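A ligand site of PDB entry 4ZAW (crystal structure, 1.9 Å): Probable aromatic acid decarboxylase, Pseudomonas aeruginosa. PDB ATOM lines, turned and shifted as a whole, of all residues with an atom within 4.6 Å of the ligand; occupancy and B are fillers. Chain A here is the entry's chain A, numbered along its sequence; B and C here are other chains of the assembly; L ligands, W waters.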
ATOM      1  N   THR A  12       6.036  26.442  16.167  1.00  0.00           N
ATOM      2  CA  THR A  12       5.613  26.641  17.564  1.00  0.00           C
ATOM      3  C   THR A  12       6.265  25.614  18.482  1.00  0.00           C
ATOM      4  O   THR A  12       7.015  24.696  18.024  1.00  0.00           O
ATOM      5  CB  THR A  12       4.056  26.689  17.757  1.00  0.00           C
ATOM      6  OG1 THR A  12       3.463  25.395  17.519  1.00  0.00           O
ATOM      7  CG2 THR A  12       3.489  27.756  16.854  1.00  0.00           C
ATOM      8  N   GLY A  13       6.068  25.815  19.757  1.00  0.00           N
ATOM      9  CA  GLY A  13       6.908  25.183  20.769  1.00  0.00           C
ATOM     10  C   GLY A  13       6.663  23.737  21.146  1.00  0.00           C
ATOM     11  O   GLY A  13       6.550  23.422  22.310  1.00  0.00           O
ATOM     12  N   ALA A  14       6.555  22.844  20.160  1.00  0.00           N
ATOM     13  CA  ALA A  14       6.643  21.418  20.410  1.00  0.00           C
ATOM     14  C   ALA A  14       7.996  20.873  19.946  1.00  0.00           C
ATOM     15  O   ALA A  14       8.661  21.449  19.074  1.00  0.00           O
ATOM     16  CB  ALA A  14       5.529  20.691  19.691  1.00  0.00           C
ATOM     17  N   SER A  15       8.373  19.758  20.521  1.00  0.00           N
ATOM     18  CA  SER A  15       9.528  18.982  20.054  1.00  0.00           C
ATOM     19  C   SER A  15       9.385  18.684  18.592  1.00  0.00           C
ATOM     20  O   SER A  15       8.284  18.434  18.095  1.00  0.00           O
ATOM     21  CB  SER A  15       9.697  17.665  20.807  1.00  0.00           C
ATOM     22  OG  SER A  15      11.032  17.206  20.525  1.00  0.00           O
ATOM     23  N   SER A  39       7.407  31.108  17.163  1.00  0.00           N
ATOM     24  CA  SER A  39       7.006  31.560  18.492  1.00  0.00           C
ATOM     25  C   SER A  39       8.213  31.613  19.435  1.00  0.00           C
ATOM     26  O   SER A  39       9.257  31.009  19.164  1.00  0.00           O
ATOM     27  CB  SER A  39       5.974  30.621  19.073  1.00  0.00           C
ATOM     28  OG  SER A  39       6.510  29.418  19.549  1.00  0.00           O
ATOM     29  N   ALA A  41       8.431  30.240  22.421  1.00  0.00           N
ATOM     30  CA  ALA A  41       8.729  28.871  22.878  1.00  0.00           C
ATOM     31  C   ALA A  41       9.413  28.003  21.811  1.00  0.00           C
ATOM     32  O   ALA A  41      10.287  27.223  22.146  1.00  0.00           O
ATOM     33  CB  ALA A  41       7.477  28.175  23.443  1.00  0.00           C
ATOM     34  N   ALA A  42       9.076  28.171  20.535  1.00  0.00           N
ATOM     35  CA  ALA A  42       9.717  27.404  19.506  1.00  0.00           C
ATOM     36  C   ALA A  42      11.252  27.789  19.406  1.00  0.00           C
ATOM     37  O   ALA A  42      12.076  26.912  19.010  1.00  0.00           O
ATOM     38  CB  ALA A  42       9.098  27.664  18.182  1.00  0.00           C
ATOM     39  N   LEU A  44      13.092  28.535  21.895  1.00  0.00           N
ATOM     40  CA  LEU A  44      13.687  27.769  22.978  1.00  0.00           C
ATOM     41  C   LEU A  44      13.834  26.314  22.651  1.00  0.00           C
ATOM     42  O   LEU A  44      14.888  25.678  22.895  1.00  0.00           O
ATOM     43  CB  LEU A  44      12.897  27.865  24.266  1.00  0.00           C
ATOM     44  CG  LEU A  44      12.623  29.272  24.741  1.00  0.00           C
ATOM     45  CD1 LEU A  44      11.663  29.248  25.937  1.00  0.00           C
ATOM     46  CD2 LEU A  44      13.926  30.003  25.090  1.00  0.00           C
ATOM     47  N   VAL A  45      12.821  25.750  22.002  1.00  0.00           N
ATOM     48  CA  VAL A  45      12.956  24.405  21.597  1.00  0.00           C
ATOM     49  C   VAL A  45      14.150  24.254  20.620  1.00  0.00           C
ATOM     50  O   VAL A  45      14.930  23.273  20.708  1.00  0.00           O
ATOM     51  CB  VAL A  45      11.647  23.876  20.940  1.00  0.00           C
ATOM     52  CG1 VAL A  45      11.883  22.519  20.321  1.00  0.00           C
ATOM     53  CG2 VAL A  45      10.502  23.822  21.967  1.00  0.00           C
ATOM     54  N   THR A  48      17.402  24.237  22.451  1.00  0.00           N
ATOM     55  CA  THR A  48      17.555  23.028  23.265  1.00  0.00           C
ATOM     56  C   THR A  48      17.871  21.819  22.459  1.00  0.00           C
ATOM     57  O   THR A  48      18.646  21.044  22.876  1.00  0.00           O
ATOM     58  CB  THR A  48      16.276  22.702  24.074  1.00  0.00           C
ATOM     59  OG1 THR A  48      15.896  23.840  24.850  1.00  0.00           O
ATOM     60  CG2 THR A  48      16.487  21.569  24.996  1.00  0.00           C
ATOM     61  N   GLU A  49      17.273  21.606  21.295  1.00  0.00           N
ATOM     62  CA  GLU A  49      17.381  20.310  20.698  1.00  0.00           C
ATOM     63  C   GLU A  49      18.059  20.337  19.335  1.00  0.00           C
ATOM     64  O   GLU A  49      18.250  19.320  18.742  1.00  0.00           O
ATOM     65  CB  GLU A  49      16.002  19.547  20.744  1.00  0.00           C
ATOM     66  CG  GLU A  49      14.923  20.047  19.834  1.00  0.00           C
ATOM     67  CD  GLU A  49      13.570  19.235  19.803  1.00  0.00           C
ATOM     68  OE1 GLU A  49      13.075  19.201  18.646  1.00  0.00           O
ATOM     69  OE2 GLU A  49      13.041  18.706  20.841  1.00  0.00           O
ATOM     70  N   SER A 104       2.427  23.089  18.767  1.00  0.00           N
ATOM     71  CA  SER A 104       2.239  22.862  20.197  1.00  0.00           C
ATOM     72  C   SER A 104       0.749  22.638  20.564  1.00  0.00           C
ATOM     73  O   SER A 104      -0.167  23.054  19.833  1.00  0.00           O
ATOM     74  CB  SER A 104       2.710  24.053  20.996  1.00  0.00           C
ATOM     75  OG  SER A 104       1.812  25.139  20.933  1.00  0.00           O
ATOM     76  N   THR A 105       0.528  21.963  21.687  1.00  0.00           N
ATOM     77  CA  THR A 105      -0.857  21.794  22.202  1.00  0.00           C
ATOM     78  C   THR A 105      -1.480  23.183  22.516  1.00  0.00           C
ATOM     79  O   THR A 105      -2.690  23.361  22.364  1.00  0.00           O
ATOM     80  CB  THR A 105      -0.960  20.821  23.361  1.00  0.00           C
ATOM     81  OG1 THR A 105      -0.377  21.362  24.559  1.00  0.00           O
ATOM     82  CG2 THR A 105      -0.339  19.475  22.996  1.00  0.00           C
ATOM     83  N   GLY A 106      -0.653  24.145  22.939  1.00  0.00           N
ATOM     84  CA  GLY A 106      -1.131  25.539  23.185  1.00  0.00           C
ATOM     85  C   GLY A 106      -1.604  26.210  21.928  1.00  0.00           C
ATOM     86  O   GLY A 106      -2.603  26.898  21.960  1.00  0.00           O
ATOM     87  N   THR A 107      -0.861  26.063  20.832  1.00  0.00           N
ATOM     88  CA  THR A 107      -1.256  26.666  19.569  1.00  0.00           C
ATOM     89  C   THR A 107      -2.484  25.924  18.979  1.00  0.00           C
ATOM     90  O   THR A 107      -3.450  26.537  18.516  1.00  0.00           O
ATOM     91  CB  THR A 107      -0.083  26.804  18.588  1.00  0.00           C
ATOM     92  OG1 THR A 107       0.776  27.906  18.965  1.00  0.00           O
ATOM     93  CG2 THR A 107      -0.629  27.100  17.218  1.00  0.00           C
ATOM     94  N   ARG A 139       3.023  17.390  17.964  1.00  0.00           N
ATOM     95  CA  ARG A 139       3.981  16.400  18.543  1.00  0.00           C
ATOM     96  C   ARG A 139       3.778  16.403  20.060  1.00  0.00           C
ATOM     97  O   ARG A 139       4.224  17.323  20.767  1.00  0.00           O
ATOM     98  CB  ARG A 139       5.442  16.764  18.136  1.00  0.00           C
ATOM     99  CG  ARG A 139       6.458  15.611  18.183  1.00  0.00           C
ATOM    100  CD  ARG A 139       6.500  14.740  19.436  1.00  0.00           C
ATOM    101  NE  ARG A 139       6.651  15.464  20.670  1.00  0.00           N
ATOM    102  CZ  ARG A 139       6.564  14.899  21.877  1.00  0.00           C
ATOM    103  NH1 ARG A 139       6.345  13.587  22.021  1.00  0.00           N
ATOM    104  NH2 ARG A 139       6.560  15.686  22.939  1.00  0.00           N
ATOM    105  N   GLU A 140       3.087  15.358  20.531  1.00  0.00           N
ATOM    106  CA  GLU A 140       2.754  15.210  21.925  1.00  0.00           C
ATOM    107  C   GLU A 140       2.402  13.765  22.129  1.00  0.00           C
ATOM    108  O   GLU A 140       1.942  13.092  21.232  1.00  0.00           O
ATOM    109  CB  GLU A 140       1.597  16.117  22.291  1.00  0.00           C
ATOM    110  CG  GLU A 140       1.127  16.081  23.767  1.00  0.00           C
ATOM    111  CD  GLU A 140       2.236  16.445  24.709  1.00  0.00           C
ATOM    112  OE1 GLU A 140       3.149  15.565  24.984  1.00  0.00           O
ATOM    113  OE2 GLU A 140       2.202  17.596  25.154  1.00  0.00           O
ATOM    114  N   TRP B  84      10.160  26.446  31.279  1.00  0.00           N
ATOM    115  CA  TRP B  84       9.822  25.198  30.589  1.00  0.00           C
ATOM    116  C   TRP B  84      10.795  24.047  30.894  1.00  0.00           C
ATOM    117  O   TRP B  84      10.517  22.904  30.546  1.00  0.00           O
ATOM    118  CB  TRP B  84       9.688  25.423  29.061  1.00  0.00           C
ATOM    119  CG  TRP B  84       8.794  26.575  28.733  1.00  0.00           C
ATOM    120  CD1 TRP B  84       9.166  27.775  28.266  1.00  0.00           C
ATOM    121  CD2 TRP B  84       7.376  26.670  28.945  1.00  0.00           C
ATOM    122  NE1 TRP B  84       8.094  28.594  28.152  1.00  0.00           N
ATOM    123  CE2 TRP B  84       6.976  27.941  28.559  1.00  0.00           C
ATOM    124  CE3 TRP B  84       6.401  25.753  29.422  1.00  0.00           C
ATOM    125  CZ2 TRP B  84       5.656  28.376  28.622  1.00  0.00           C
ATOM    126  CZ3 TRP B  84       5.082  26.197  29.481  1.00  0.00           C
ATOM    127  CH2 TRP B  84       4.716  27.498  29.072  1.00  0.00           C
ATOM    128  N   MET B  85      11.932  24.326  31.537  1.00  0.00           N
ATOM    129  CA  MET B  85      12.853  23.252  31.971  1.00  0.00           C
ATOM    130  C   MET B  85      12.511  22.617  33.337  1.00  0.00           C
ATOM    131  O   MET B  85      13.154  21.692  33.776  1.00  0.00           O
ATOM    132  CB  MET B  85      14.297  23.827  32.042  1.00  0.00           C
ATOM    133  CG  MET B  85      14.785  24.519  30.768  1.00  0.00           C
ATOM    134  SD  MET B  85      14.573  23.575  29.205  1.00  0.00           S
ATOM    135  CE  MET B  85      14.210  24.964  28.073  1.00  0.00           C
ATOM    136  N   CYS B 116      -2.354  26.351  27.744  1.00  0.00           N
ATOM    137  CA  CYS B 116      -0.954  26.144  28.101  1.00  0.00           C
ATOM    138  C   CYS B 116      -0.102  27.417  27.981  1.00  0.00           C
ATOM    139  O   CYS B 116       1.041  27.356  27.497  1.00  0.00           O
ATOM    140  CB  CYS B 116      -0.349  25.106  27.196  1.00  0.00           C
ATOM    141  SG  CYS B 116      -0.878  23.421  27.407  1.00  0.00           S
ATOM    142  N   ASN B 117      -0.621  28.556  28.358  1.00  0.00           N
ATOM    143  CA  ASN B 117       0.123  29.802  28.146  1.00  0.00           C
ATOM    144  C   ASN B 117       1.260  30.062  29.135  1.00  0.00           C
ATOM    145  O   ASN B 117       2.007  30.950  28.916  1.00  0.00           O
ATOM    146  CB  ASN B 117      -0.792  31.015  28.281  1.00  0.00           C
ATOM    147  CG  ASN B 117      -1.840  31.105  27.142  1.00  0.00           C
ATOM    148  OD1 ASN B 117      -1.498  30.975  25.942  1.00  0.00           O
ATOM    149  ND2 ASN B 117      -3.108  31.340  27.533  1.00  0.00           N
ATOM    150  N   ARG B 122       0.339  24.786  31.500  1.00  0.00           N
ATOM    151  CA  ARG B 122       0.945  23.601  30.926  1.00  0.00           C
ATOM    152  C   ARG B 122       1.044  22.454  31.930  1.00  0.00           C
ATOM    153  O   ARG B 122       0.851  21.283  31.570  1.00  0.00           O
ATOM    154  CB  ARG B 122       2.342  23.921  30.354  1.00  0.00           C
ATOM    155  CG  ARG B 122       3.129  22.705  29.887  1.00  0.00           C
ATOM    156  CD  ARG B 122       2.454  22.011  28.712  1.00  0.00           C
ATOM    157  NE  ARG B 122       3.308  20.966  28.176  1.00  0.00           N
ATOM    158  CZ  ARG B 122       2.963  20.122  27.205  1.00  0.00           C
ATOM    159  NH1 ARG B 122       1.740  20.121  26.660  1.00  0.00           N
ATOM    160  NH2 ARG B 122       3.892  19.282  26.775  1.00  0.00           N
ATOM    161  N   TYR C 169      14.082  15.656  22.196  1.00  0.00           N
ATOM    162  CA  TYR C 169      14.749  16.426  23.195  1.00  0.00           C
ATOM    163  C   TYR C 169      15.735  15.618  24.081  1.00  0.00           C
ATOM    164  O   TYR C 169      16.177  16.156  25.041  1.00  0.00           O
ATOM    165  CB  TYR C 169      13.738  17.205  24.023  1.00  0.00           C
ATOM    166  CG  TYR C 169      12.617  16.435  24.704  1.00  0.00           C
ATOM    167  CD1 TYR C 169      12.779  15.922  25.951  1.00  0.00           C
ATOM    168  CD2 TYR C 169      11.412  16.243  24.089  1.00  0.00           C
ATOM    169  CE1 TYR C 169      11.762  15.240  26.588  1.00  0.00           C
ATOM    170  CE2 TYR C 169      10.358  15.593  24.712  1.00  0.00           C
ATOM    171  CZ  TYR C 169      10.523  15.107  25.946  1.00  0.00           C
ATOM    172  OH  TYR C 169       9.478  14.460  26.555  1.00  0.00           O
ATOM    173  N   TRP C 200      12.386  14.463  33.427  1.00  0.00           N
ATOM    174  CA  TRP C 200      12.564  15.872  33.120  1.00  0.00           C
ATOM    175  C   TRP C 200      12.697  16.804  34.294  1.00  0.00           C
ATOM    176  O   TRP C 200      11.876  16.803  35.216  1.00  0.00           O
ATOM    177  CB  TRP C 200      11.410  16.361  32.213  1.00  0.00           C
ATOM    178  CG  TRP C 200      11.590  17.698  31.677  1.00  0.00           C
ATOM    179  CD1 TRP C 200      10.939  18.839  32.069  1.00  0.00           C
ATOM    180  CD2 TRP C 200      12.493  18.093  30.622  1.00  0.00           C
ATOM    181  NE1 TRP C 200      11.373  19.904  31.327  1.00  0.00           N
ATOM    182  CE2 TRP C 200      12.334  19.478  30.432  1.00  0.00           C
ATOM    183  CE3 TRP C 200      13.459  17.428  29.860  1.00  0.00           C
ATOM    184  CZ2 TRP C 200      13.074  20.199  29.510  1.00  0.00           C
ATOM    185  CZ3 TRP C 200      14.148  18.124  28.918  1.00  0.00           C
ATOM    186  CH2 TRP C 200      13.956  19.503  28.729  1.00  0.00           C
HETATM  187  C1  LIG L   1       8.167  23.709  25.619  1.00  0.00           C
HETATM  188  C2  LIG L   1       9.569  23.886  25.656  1.00  0.00           C
HETATM  189  C3  LIG L   1      10.414  22.788  25.460  1.00  0.00           C
HETATM  190  C4  LIG L   1       5.728  21.322  24.476  1.00  0.00           C
HETATM  191  C5  LIG L   1       9.853  21.497  25.166  1.00  0.00           C
HETATM  192  N1  LIG L   1       4.732  19.444  22.781  1.00  0.00           N
HETATM  193  C6  LIG L   1       3.924  20.410  23.158  1.00  0.00           C
HETATM  194  C7  LIG L   1      11.135  19.980  23.627  1.00  0.00           C
HETATM  195  C8  LIG L   1      10.611  20.283  25.032  1.00  0.00           C
HETATM  196  C9  LIG L   1       8.526  18.949  24.669  1.00  0.00           C
HETATM  197  O1  LIG L   1       2.767  20.478  22.711  1.00  0.00           O
HETATM  198  N2  LIG L   1       4.391  21.348  24.009  1.00  0.00           N
HETATM  199  C10 LIG L   1       6.091  19.355  23.168  1.00  0.00           C
HETATM  200  O2  LIG L   1       6.750  18.409  22.647  1.00  0.00           O
HETATM  201  C11 LIG L   1       6.593  20.297  24.086  1.00  0.00           C
HETATM  202  N3  LIG L   1       7.771  20.175  24.808  1.00  0.00           N
HETATM  203  C12 LIG L   1       9.756  19.131  25.584  1.00  0.00           C
HETATM  204  C13 LIG L   1      11.859  20.205  26.063  1.00  0.00           C
HETATM  205  C14 LIG L   1       8.409  21.361  25.135  1.00  0.00           C
HETATM  206  C15 LIG L   1      11.834  23.053  25.331  1.00  0.00           C
HETATM  207  C16 LIG L   1      10.027  25.278  25.679  1.00  0.00           C
HETATM  208  C17 LIG L   1       7.584  22.458  25.382  1.00  0.00           C
HETATM  209  N4  LIG L   1       6.200  22.311  25.293  1.00  0.00           N
HETATM  210  C18 LIG L   1       5.254  23.393  25.739  1.00  0.00           C
HETATM  211  C19 LIG L   1       4.948  24.542  24.849  1.00  0.00           C
HETATM  212  O3  LIG L   1       6.114  25.212  24.298  1.00  0.00           O
HETATM  213  C20 LIG L   1       4.066  25.553  25.543  1.00  0.00           C
HETATM  214  O4  LIG L   1       2.962  25.111  26.317  1.00  0.00           O
HETATM  215  C21 LIG L   1       4.133  26.958  25.100  1.00  0.00           C
HETATM  216  O5  LIG L   1       3.330  27.843  25.857  1.00  0.00           O
HETATM  217  C22 LIG L   1       3.590  26.942  23.725  1.00  0.00           C
HETATM  218  O6  LIG L   1       3.624  28.270  23.201  1.00  0.00           O
HETATM  219  P1  LIG L   1       3.614  28.382  21.584  1.00  0.00           P
HETATM  220  O7  LIG L   1       2.372  27.592  21.029  1.00  0.00           O
HETATM  221  O8  LIG L   1       3.362  29.881  21.374  1.00  0.00           O
HETATM  222  O9  LIG L   1       4.875  27.918  20.933  1.00  0.00           O
HETATM  223  O   HOH W   1       1.905  23.048  24.515  1.00  0.00           O
HETATM  224  O   HOH W   2       5.672  31.164  22.727  1.00  0.00           O
HETATM  225  O   HOH W   3       1.782  19.136  19.989  1.00  0.00           O
HETATM  226  O   HOH W   4       0.013  28.962  22.132  1.00  0.00           O
HETATM  227  O   HOH W   5       0.716  28.267  24.490  1.00  0.00           O
HETATM  228  O   HOH W   6       1.903  30.682  19.032  1.00  0.00           O
HETATM  229  O   HOH W   7       3.514  30.500  26.144  1.00  0.00           O
HETATM  230  O   HOH W   8       6.589  19.692  27.520  1.00  0.00           O
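A nitrogen (N2) of the ligand sits close to the guanidinium group of Arg 122 of chain B, 3.5 Å away.
Merely in contact with the ligand: Thr 12 (3.5 Å), Ala 14 (3.4 Å), Ala 41 (3.4 Å), Val 45 (3.6 Å), Glu 49 (3.6 Å), Glu 140 (3.8 Å), Trp 84 of chain B (3.4 Å), Tyr 169 of chain C (3.6 Å) and Trp 200 of chain C (3.5 Å).
Hydrophobic or aromatic side chains within 4 Å of the ligand: Ala 14, Ala 41, Val 45, Trp 84 of chain B, Tyr 169 of chain C and Trp 200 of chain C.
Of the 24 residues printed, 18 come within 4 Å of the ligand.
The nearest printed residue that does not touch the ligand is Met 85 of chain B (4.1 Å).
NH2 of Arg 139 is in hydrogen-bond range of O2 of the ligand.
O of Cys 116 of chain B sits at hydrogen-bond distance from O5 of the ligand (2.9 Å).
An oxygen (O7) of the ligand lies within hydrogen-bond range of the side-chain hydroxyl of Thr 107 (2.6 Å).
The backbone NH of Ser 15 is in hydrogen-bond range of an oxygen (O2) of the ligand (3.0 Å).
O of Arg 139 is in hydrogen-bond range of N1 of the ligand (3.0 Å).
O3 of the ligand is in hydrogen-bond range of O of Gly 13 (2.7 Å).
N of Thr 105 sits at hydrogen-bond distance from O1 of the ligand, 2.9 Å away.
An oxygen (O9) of the ligand is in hydrogen-bond range of the side-chain hydroxyl (OG) of Ser 39, at 2.6 Å.
O9 of the ligand sits at hydrogen-bond distance from N of Gly 13, 2.7 Å away.
The side-chain hydroxyl of Ser 104 sits at hydrogen-bond distance from an oxygen (O7) of the ligand (2.5 Å).
Water W7 bridges an oxygen (O5) of the ligand and the backbone carbonyl oxygen of Asn 117 of chain B.
Water W6 lies within hydrogen-bond range of O8 of the ligand (2.9 Å) and OG1 of Thr 107 (3.0 Å).
Water W1 lies within hydrogen-bond range of OG1 of Thr 105 (2.8 Å), O4 of the ligand (2.9 Å) and N of Gly 106 (3.2 Å).
Water W4 lies within hydrogen-bond range of O7 of the ligand, N of Thr 107 and O of Gly 106.
Water W2 lies within hydrogen-bond range of the backbone NH (N) of Ala 41 (2.9 Å) and an oxygen (O8) of the ligand (3.0 Å).
Water W5 bridges O5 of the ligand (3.0 Å) and O of Cys 116 of chain B (3.2 Å).
The backbone NH (N) of Ser 104 is in hydrogen-bond range of the side-chain hydroxyl (OG1) of Thr 12, at 2.8 Å.
The side-chain carboxylate of Glu 140 is in salt-bridge range of the guanidinium group of Arg 139, 3.98 Å away.
The side-chain hydroxyl (OG) of Ser 104 sits close to the backbone NH (N) of Gly 106.
The side-chain hydroxyl (OG) of Ser 15 lies within hydrogen-bond range of the side-chain carboxylate (OE2) of Glu 49, at 2.5 Å.
The side-chain hydroxyl of Thr 105 is in hydrogen-bond range of the guanidinium group of Arg 122 of chain B.
OE2 of Glu 49 lies within hydrogen-bond range of N of Tyr 169 of chain C (3.5 Å).
The guanidinium group (NH2) of Arg 122 of chain B is in salt-bridge range of the side-chain carboxylate (OE2) of Glu 140 (2.9 Å).
The side-chain sulfur (SG) of Cys 116 of chain B sits at hydrogen-bond distance from the side-chain hydroxyl (OG1) of Thr 105 (3.5 Å).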
